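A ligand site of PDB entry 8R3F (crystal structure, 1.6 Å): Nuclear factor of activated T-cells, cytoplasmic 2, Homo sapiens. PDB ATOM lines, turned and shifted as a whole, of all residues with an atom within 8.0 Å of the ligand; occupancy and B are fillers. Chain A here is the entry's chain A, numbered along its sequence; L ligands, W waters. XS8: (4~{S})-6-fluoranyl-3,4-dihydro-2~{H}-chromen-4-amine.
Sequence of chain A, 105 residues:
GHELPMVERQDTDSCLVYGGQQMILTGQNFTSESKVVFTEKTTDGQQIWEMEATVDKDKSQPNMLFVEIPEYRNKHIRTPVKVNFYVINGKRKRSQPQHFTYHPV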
ATOM      1  N   ASN A  29     -17.244  24.024 -21.397  1.00  0.00           N
ATOM      2  CA  ASN A  29     -16.957  22.582 -21.451  1.00  0.00           C
ATOM      3  C   ASN A  29     -17.690  21.794 -20.360  1.00  0.00           C
ATOM      4  O   ASN A  29     -17.177  20.782 -19.878  1.00  0.00           O
ATOM      5  CB  ASN A  29     -15.448  22.305 -21.382  1.00  0.00           C
ATOM      6  CG  ASN A  29     -14.680  23.022 -22.482  1.00  0.00           C
ATOM      7  OD1 ASN A  29     -15.140  23.048 -23.631  1.00  0.00           O
ATOM      8  ND2 ASN A  29     -13.512  23.572 -22.161  1.00  0.00           N
ATOM      9  N   PHE A  30     -18.869  22.250 -19.959  1.00  0.00           N
ATOM     10  CA  PHE A  30     -19.733  21.452 -19.085  1.00  0.00           C
ATOM     11  C   PHE A  30     -20.523  20.429 -19.900  1.00  0.00           C
ATOM     12  O   PHE A  30     -20.945  20.683 -21.021  1.00  0.00           O
ATOM     13  CB  PHE A  30     -20.723  22.354 -18.368  1.00  0.00           C
ATOM     14  CG  PHE A  30     -20.111  23.495 -17.602  1.00  0.00           C
ATOM     15  CD1 PHE A  30     -18.908  23.331 -16.918  1.00  0.00           C
ATOM     16  CD2 PHE A  30     -20.777  24.722 -17.527  1.00  0.00           C
ATOM     17  CE1 PHE A  30     -18.360  24.375 -16.195  1.00  0.00           C
ATOM     18  CE2 PHE A  30     -20.267  25.749 -16.814  1.00  0.00           C
ATOM     19  CZ  PHE A  30     -19.054  25.593 -16.118  1.00  0.00           C
ATOM     20  N   THR A  31     -20.772  19.263 -19.300  1.00  0.00           N
ATOM     21  CA  THR A  31     -21.564  18.227 -19.934  1.00  0.00           C
ATOM     22  C   THR A  31     -22.496  17.620 -18.897  1.00  0.00           C
ATOM     23  O   THR A  31     -22.380  17.895 -17.704  1.00  0.00           O
ATOM     24  CB  THR A  31     -20.688  17.107 -20.501  1.00  0.00           C
ATOM     25  OG1 THR A  31     -20.233  16.333 -19.375  1.00  0.00           O
ATOM     26  CG2 THR A  31     -19.513  17.645 -21.277  1.00  0.00           C
ATOM     27  N   SER A  32     -23.393  16.748 -19.363  1.00  0.00           N
ATOM     28  CA  SER A  32     -24.256  16.046 -18.417  1.00  0.00           C
ATOM     29  C   SER A  32     -23.491  15.078 -17.512  1.00  0.00           C
ATOM     30  O   SER A  32     -24.087  14.471 -16.619  1.00  0.00           O
ATOM     31  CB  SER A  32     -25.357  15.289 -19.164  1.00  0.00           C
ATOM     32  OG  SER A  32     -24.825  14.290 -20.015  1.00  0.00           O
ATOM     33  N   GLU A  33     -22.186  14.904 -17.732  1.00  0.00           N
ATOM     34  CA  GLU A  33     -21.377  14.079 -16.850  1.00  0.00           C
ATOM     35  C   GLU A  33     -20.467  14.906 -15.932  1.00  0.00           C
ATOM     36  O   GLU A  33     -19.867  14.333 -15.005  1.00  0.00           O
ATOM     37  CB  GLU A  33     -20.544  13.093 -17.674  1.00  0.00           C
ATOM     38  CG  GLU A  33     -21.406  11.967 -18.310  1.00  0.00           C
ATOM     39  CD  GLU A  33     -20.652  11.086 -19.295  1.00  0.00           C
ATOM     40  OE1 GLU A  33     -19.460  11.353 -19.563  1.00  0.00           O
ATOM     41  OE2 GLU A  33     -21.261  10.103 -19.804  1.00  0.00           O
ATOM     42  N   SER A  34     -20.411  16.225 -16.107  1.00  0.00           N
ATOM     43  CA  SER A  34     -19.695  17.076 -15.161  1.00  0.00           C
ATOM     44  C   SER A  34     -20.206  16.849 -13.752  1.00  0.00           C
ATOM     45  O   SER A  34     -21.411  16.705 -13.524  1.00  0.00           O
ATOM     46  CB  SER A  34     -19.892  18.552 -15.537  1.00  0.00           C
ATOM     47  OG  SER A  34     -19.445  18.872 -16.843  1.00  0.00           O
ATOM     48  N   LYS A  35     -19.298  16.835 -12.795  1.00  0.00           N
ATOM     49  CA  LYS A  35     -19.644  16.789 -11.383  1.00  0.00           C
ATOM     50  C   LYS A  35     -19.122  18.076 -10.750  1.00  0.00           C
ATOM     51  O   LYS A  35     -18.134  18.653 -11.222  1.00  0.00           O
ATOM     52  CB  LYS A  35     -19.036  15.553 -10.654  1.00  0.00           C
ATOM     53  CG  LYS A  35     -19.399  14.246 -11.217  1.00  0.00           C
ATOM     54  CD  LYS A  35     -18.942  13.082 -10.346  1.00  0.00           C
ATOM     55  CE  LYS A  35     -19.101  11.744 -11.076  1.00  0.00           C
ATOM     56  NZ  LYS A  35     -17.862  11.358 -11.797  1.00  0.00           N
ATOM     57  N   VAL A  55     -26.251  18.585  -9.477  1.00  0.00           N
ATOM     58  CA  VAL A  55     -26.404  19.380 -10.690  1.00  0.00           C
ATOM     59  C   VAL A  55     -27.810  19.173 -11.259  1.00  0.00           C
ATOM     60  O   VAL A  55     -28.294  18.048 -11.355  1.00  0.00           O
ATOM     61  CB  VAL A  55     -25.342  18.994 -11.737  1.00  0.00           C
ATOM     62  CG1 VAL A  55     -25.633  19.684 -13.064  1.00  0.00           C
ATOM     63  CG2 VAL A  55     -23.960  19.352 -11.287  1.00  0.00           C
ATOM     64  N   ASP A  56     -28.469  20.271 -11.646  1.00  0.00           N
ATOM     65  CA  ASP A  56     -29.747  20.213 -12.352  1.00  0.00           C
ATOM     66  C   ASP A  56     -29.437  20.015 -13.832  1.00  0.00           C
ATOM     67  O   ASP A  56     -29.141  20.972 -14.543  1.00  0.00           O
ATOM     68  CB  ASP A  56     -30.552  21.484 -12.134  1.00  0.00           C
ATOM     69  CG  ASP A  56     -31.923  21.448 -12.805  1.00  0.00           C
ATOM     70  OD1 ASP A  56     -32.102  20.727 -13.818  1.00  0.00           O
ATOM     71  OD2 ASP A  56     -32.799  22.187 -12.318  1.00  0.00           O
ATOM     72  N   LYS A  57     -29.505  18.763 -14.304  1.00  0.00           N
ATOM     73  CA  LYS A  57     -29.003  18.473 -15.647  1.00  0.00           C
ATOM     74  C   LYS A  57     -29.988  18.847 -16.738  1.00  0.00           C
ATOM     75  O   LYS A  57     -29.587  18.974 -17.894  1.00  0.00           O
ATOM     76  CB  LYS A  57     -28.597  16.995 -15.754  1.00  0.00           C
ATOM     77  CG  LYS A  57     -27.667  16.539 -14.618  1.00  0.00           C
ATOM     78  CD  LYS A  57     -26.930  15.274 -14.954  1.00  0.00           C
ATOM     79  CE  LYS A  57     -25.856  14.946 -13.886  1.00  0.00           C
ATOM     80  NZ  LYS A  57     -24.500  15.390 -14.272  1.00  0.00           N
ATOM     81  N   ASP A  58     -31.244  19.080 -16.381  1.00  0.00           N
ATOM     82  CA  ASP A  58     -32.207  19.555 -17.369  1.00  0.00           C
ATOM     83  C   ASP A  58     -31.944  21.016 -17.725  1.00  0.00           C
ATOM     84  O   ASP A  58     -31.903  21.389 -18.895  1.00  0.00           O
ATOM     85  CB  ASP A  58     -33.625  19.339 -16.850  1.00  0.00           C
ATOM     86  CG  ASP A  58     -33.877  17.900 -16.451  1.00  0.00           C
ATOM     87  OD1 ASP A  58     -33.697  16.991 -17.312  1.00  0.00           O
ATOM     88  OD2 ASP A  58     -34.249  17.664 -15.274  1.00  0.00           O
ATOM     89  N   LYS A  59     -31.724  21.863 -16.720  1.00  0.00           N
ATOM     90  CA  LYS A  59     -31.520  23.285 -16.966  1.00  0.00           C
ATOM     91  C   LYS A  59     -30.127  23.631 -17.499  1.00  0.00           C
ATOM     92  O   LYS A  59     -29.952  24.686 -18.109  1.00  0.00           O
ATOM     93  CB  LYS A  59     -31.735  24.112 -15.683  1.00  0.00           C
ATOM     94  CG  LYS A  59     -33.122  24.533 -15.344  1.00  0.00           C
ATOM     95  CD  LYS A  59     -33.238  25.237 -13.976  1.00  0.00           C
ATOM     96  CE  LYS A  59     -33.300  26.783 -14.073  1.00  0.00           C
ATOM     97  NZ  LYS A  59     -33.343  27.475 -12.717  1.00  0.00           N
ATOM     98  N   SER A  60     -29.120  22.811 -17.186  1.00  0.00           N
ATOM     99  CA  SER A  60     -27.742  23.158 -17.481  1.00  0.00           C
ATOM    100  C   SER A  60     -27.433  23.036 -18.971  1.00  0.00           C
ATOM    101  O   SER A  60     -28.076  22.295 -19.719  1.00  0.00           O
ATOM    102  CB  SER A  60     -26.781  22.281 -16.657  1.00  0.00           C
ATOM    103  OG  SER A  60     -26.953  22.495 -15.272  1.00  0.00           O
ATOM    104  N   GLN A  61     -26.442  23.815 -19.388  1.00  0.00           N
ATOM    105  CA  GLN A  61     -25.995  23.953 -20.763  1.00  0.00           C
ATOM    106  C   GLN A  61     -24.471  23.891 -20.771  1.00  0.00           C
ATOM    107  O   GLN A  61     -23.820  24.054 -19.733  1.00  0.00           O
ATOM    108  CB  GLN A  61     -26.446  25.297 -21.371  1.00  0.00           C
ATOM    109  CG  GLN A  61     -27.976  25.494 -21.459  1.00  0.00           C
ATOM    110  CD  GLN A  61     -28.645  24.457 -22.311  1.00  0.00           C
ATOM    111  OE1 GLN A  61     -28.159  24.145 -23.409  1.00  0.00           O
ATOM    112  NE2 GLN A  61     -29.785  23.914 -21.843  1.00  0.00           N
ATOM    113  N   PRO A  62     -23.858  23.734 -21.952  1.00  0.00           N
ATOM    114  CA  PRO A  62     -22.391  23.597 -21.973  1.00  0.00           C
ATOM    115  C   PRO A  62     -21.646  24.771 -21.375  1.00  0.00           C
ATOM    116  O   PRO A  62     -20.520  24.564 -20.899  1.00  0.00           O
ATOM    117  CB  PRO A  62     -22.070  23.425 -23.478  1.00  0.00           C
ATOM    118  CG  PRO A  62     -23.359  23.002 -24.139  1.00  0.00           C
ATOM    119  CD  PRO A  62     -24.468  23.640 -23.294  1.00  0.00           C
ATOM    120  N   ASN A  63     -22.251  25.971 -21.301  1.00  0.00           N
ATOM    121  CA  ASN A  63     -21.607  27.135 -20.696  1.00  0.00           C
ATOM    122  C   ASN A  63     -22.287  27.588 -19.393  1.00  0.00           C
ATOM    123  O   ASN A  63     -21.937  28.645 -18.852  1.00  0.00           O
ATOM    124  CB  ASN A  63     -21.567  28.321 -21.664  1.00  0.00           C
ATOM    125  CG  ASN A  63     -20.800  28.030 -22.946  1.00  0.00           C
ATOM    126  OD1 ASN A  63     -19.999  27.117 -23.023  1.00  0.00           O
ATOM    127  ND2 ASN A  63     -21.074  28.822 -23.971  1.00  0.00           N
ATOM    128  N   MET A  64     -23.247  26.806 -18.874  1.00  0.00           N
ATOM    129  CA  MET A  64     -24.037  27.227 -17.705  1.00  0.00           C
ATOM    130  C   MET A  64     -24.444  26.015 -16.854  1.00  0.00           C
ATOM    131  O   MET A  64     -25.290  25.234 -17.282  1.00  0.00           O
ATOM    132  CB  MET A  64     -25.299  27.955 -18.194  1.00  0.00           C
ATOM    133  CG  MET A  64     -25.998  28.894 -17.249  1.00  0.00           C
ATOM    134  SD  MET A  64     -27.273  29.883 -18.118  1.00  0.00           S
ATOM    135  CE  MET A  64     -28.018  28.651 -19.156  1.00  0.00           C
ATOM    136  N   LEU A  65     -23.918  25.913 -15.635  1.00  0.00           N
ATOM    137  CA  LEU A  65     -24.239  24.812 -14.726  1.00  0.00           C
ATOM    138  C   LEU A  65     -25.082  25.312 -13.556  1.00  0.00           C
ATOM    139  O   LEU A  65     -24.714  26.285 -12.906  1.00  0.00           O
ATOM    140  CB  LEU A  65     -22.993  24.135 -14.146  1.00  0.00           C
ATOM    141  CG  LEU A  65     -22.312  22.988 -14.839  1.00  0.00           C
ATOM    142  CD1 LEU A  65     -21.098  22.537 -14.025  1.00  0.00           C
ATOM    143  CD2 LEU A  65     -23.251  21.839 -15.087  1.00  0.00           C
ATOM    144  N   PHE A  66     -26.175  24.628 -13.285  1.00  0.00           N
ATOM    145  CA  PHE A  66     -27.070  24.914 -12.176  1.00  0.00           C
ATOM    146  C   PHE A  66     -26.784  23.894 -11.069  1.00  0.00           C
ATOM    147  O   PHE A  66     -26.967  22.689 -11.278  1.00  0.00           O
ATOM    148  CB  PHE A  66     -28.523  24.826 -12.654  1.00  0.00           C
ATOM    149  CG  PHE A  66     -28.912  25.946 -13.552  1.00  0.00           C
ATOM    150  CD1 PHE A  66     -28.571  25.902 -14.907  1.00  0.00           C
ATOM    151  CD2 PHE A  66     -29.597  27.038 -13.078  1.00  0.00           C
ATOM    152  CE1 PHE A  66     -28.900  26.914 -15.750  1.00  0.00           C
ATOM    153  CE2 PHE A  66     -29.948  28.078 -13.949  1.00  0.00           C
ATOM    154  CZ  PHE A  66     -29.596  28.011 -15.271  1.00  0.00           C
ATOM    155  N   ASN A  89     -14.658  16.768 -15.021  1.00  0.00           N
ATOM    156  CA  ASN A  89     -15.071  15.900 -16.108  1.00  0.00           C
ATOM    157  C   ASN A  89     -14.154  14.682 -16.085  1.00  0.00           C
ATOM    158  O   ASN A  89     -12.926  14.813 -16.133  1.00  0.00           O
ATOM    159  CB  ASN A  89     -14.944  16.624 -17.434  1.00  0.00           C
ATOM    160  CG  ASN A  89     -16.004  17.703 -17.608  1.00  0.00           C
ATOM    161  OD1 ASN A  89     -16.992  17.784 -16.845  1.00  0.00           O
ATOM    162  ND2 ASN A  89     -15.796  18.562 -18.571  1.00  0.00           N
HETATM  163  C4  XS8 L   1     -25.454  20.269 -20.789  1.00  0.00           C
HETATM  164  C5  XS8 L   1     -26.542  19.554 -20.274  1.00  0.00           C
HETATM  165  C6  XS8 L   1     -26.520  19.205 -18.930  1.00  0.00           C
HETATM  166  C8  XS8 L   1     -26.695  20.816 -22.667  1.00  0.00           C
HETATM  167  C10 XS8 L   1     -27.745  19.164 -21.100  1.00  0.00           C
HETATM  168  C1  XS8 L   1     -25.423  19.536 -18.173  1.00  0.00           C
HETATM  169  C2  XS8 L   1     -24.359  20.253 -18.665  1.00  0.00           C
HETATM  170  C3  XS8 L   1     -24.371  20.610 -19.997  1.00  0.00           C
HETATM  171  C9  XS8 L   1     -27.532  19.572 -22.557  1.00  0.00           C
HETATM  172  F12 XS8 L   1     -25.416  19.168 -16.862  1.00  0.00           F
HETATM  173  N11 XS8 L   1     -28.978  19.824 -20.556  1.00  0.00           N
HETATM  174  O7  XS8 L   1     -25.396  20.652 -22.101  1.00  0.00           O
HETATM  175  O   HOH W   1     -22.635  19.513 -23.235  1.00  0.00           O
HETATM  176  O   HOH W   2     -23.532  17.572 -14.831  1.00  0.00           O
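Water W1 lies within hydrogen-bond range of the backbone carbonyl oxygen of Phe 30 (3.0 Å) and an oxygen (O7) of the ligand (3.2 Å).
Water W2 lies within hydrogen-bond range of NZ of Lys 57 (2.5 Å), O of Ser 34 (2.6 Å) and O of Thr 31 (3.1 Å).
The side-chain hydroxyl of Ser 60 lies within hydrogen-bond range of the backbone carbonyl oxygen of Asp 56, at 2.8 Å.
N of Phe 66 sits at hydrogen-bond distance from OG of Ser 60 (3.0 Å).
The side-chain amino group of Lys 57 is in hydrogen-bond range of the backbone carbonyl oxygen of Ser 32, at 2.6 Å.
NZ of Lys 57 sits at hydrogen-bond distance from O of Ser 34 (3.4 Å).
N of Thr 31 is in hydrogen-bond range of OG of Ser 34 (2.8 Å).
The backbone carbonyl oxygen (O) of Pro 62 lies within hydrogen-bond range of the backbone NH (N) of Phe 30 (3.0 Å).
The backbone carbonyl oxygen (O) of Pro 62 lies within hydrogen-bond range of the backbone NH (N) of Asn 29, 3.4 Å away.
OD1 of Asp 56 lies within hydrogen-bond range of N of Asp 58, at 3.2 Å.
The backbone carbonyl oxygen (O) of Thr 31 lies close to a fluorine (F12) of the ligand (3.4 Å).
N of Pro 62 sits close to O7 of the ligand (3.4 Å).
O of Phe 30 touches C3 of the ligand (3.6 Å).
N of Ser 32 touches C1 of the ligand, at 3.6 Å.
Val 55 touches the ligand.
Asp 58 touches the ligand.
Gln 61 touches the ligand.
CD2 of Leu 65 touches F12 of the ligand, at 3.9 Å.
Hydrophobic or aromatic side chains that line the ligand: Val 55, Pro 62 and Leu 65.
Within 4 Å of the ligand: Phe 30, Thr 31, Ser 32, Val 55, Lys 57, Asp 58, Ser 60, Gln 61, Pro 62 and Leu 65.
The nearest printed residue that does not touch the ligand is Asp 56 (4.7 Å).
A nitrogen (N11) of the ligand lies within hydrogen-bond range of the backbone carbonyl oxygen of Ser 60, 2.8 Å away.
N11 of the ligand sits at hydrogen-bond distance from O of Lys 57, 2.9 Å away.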
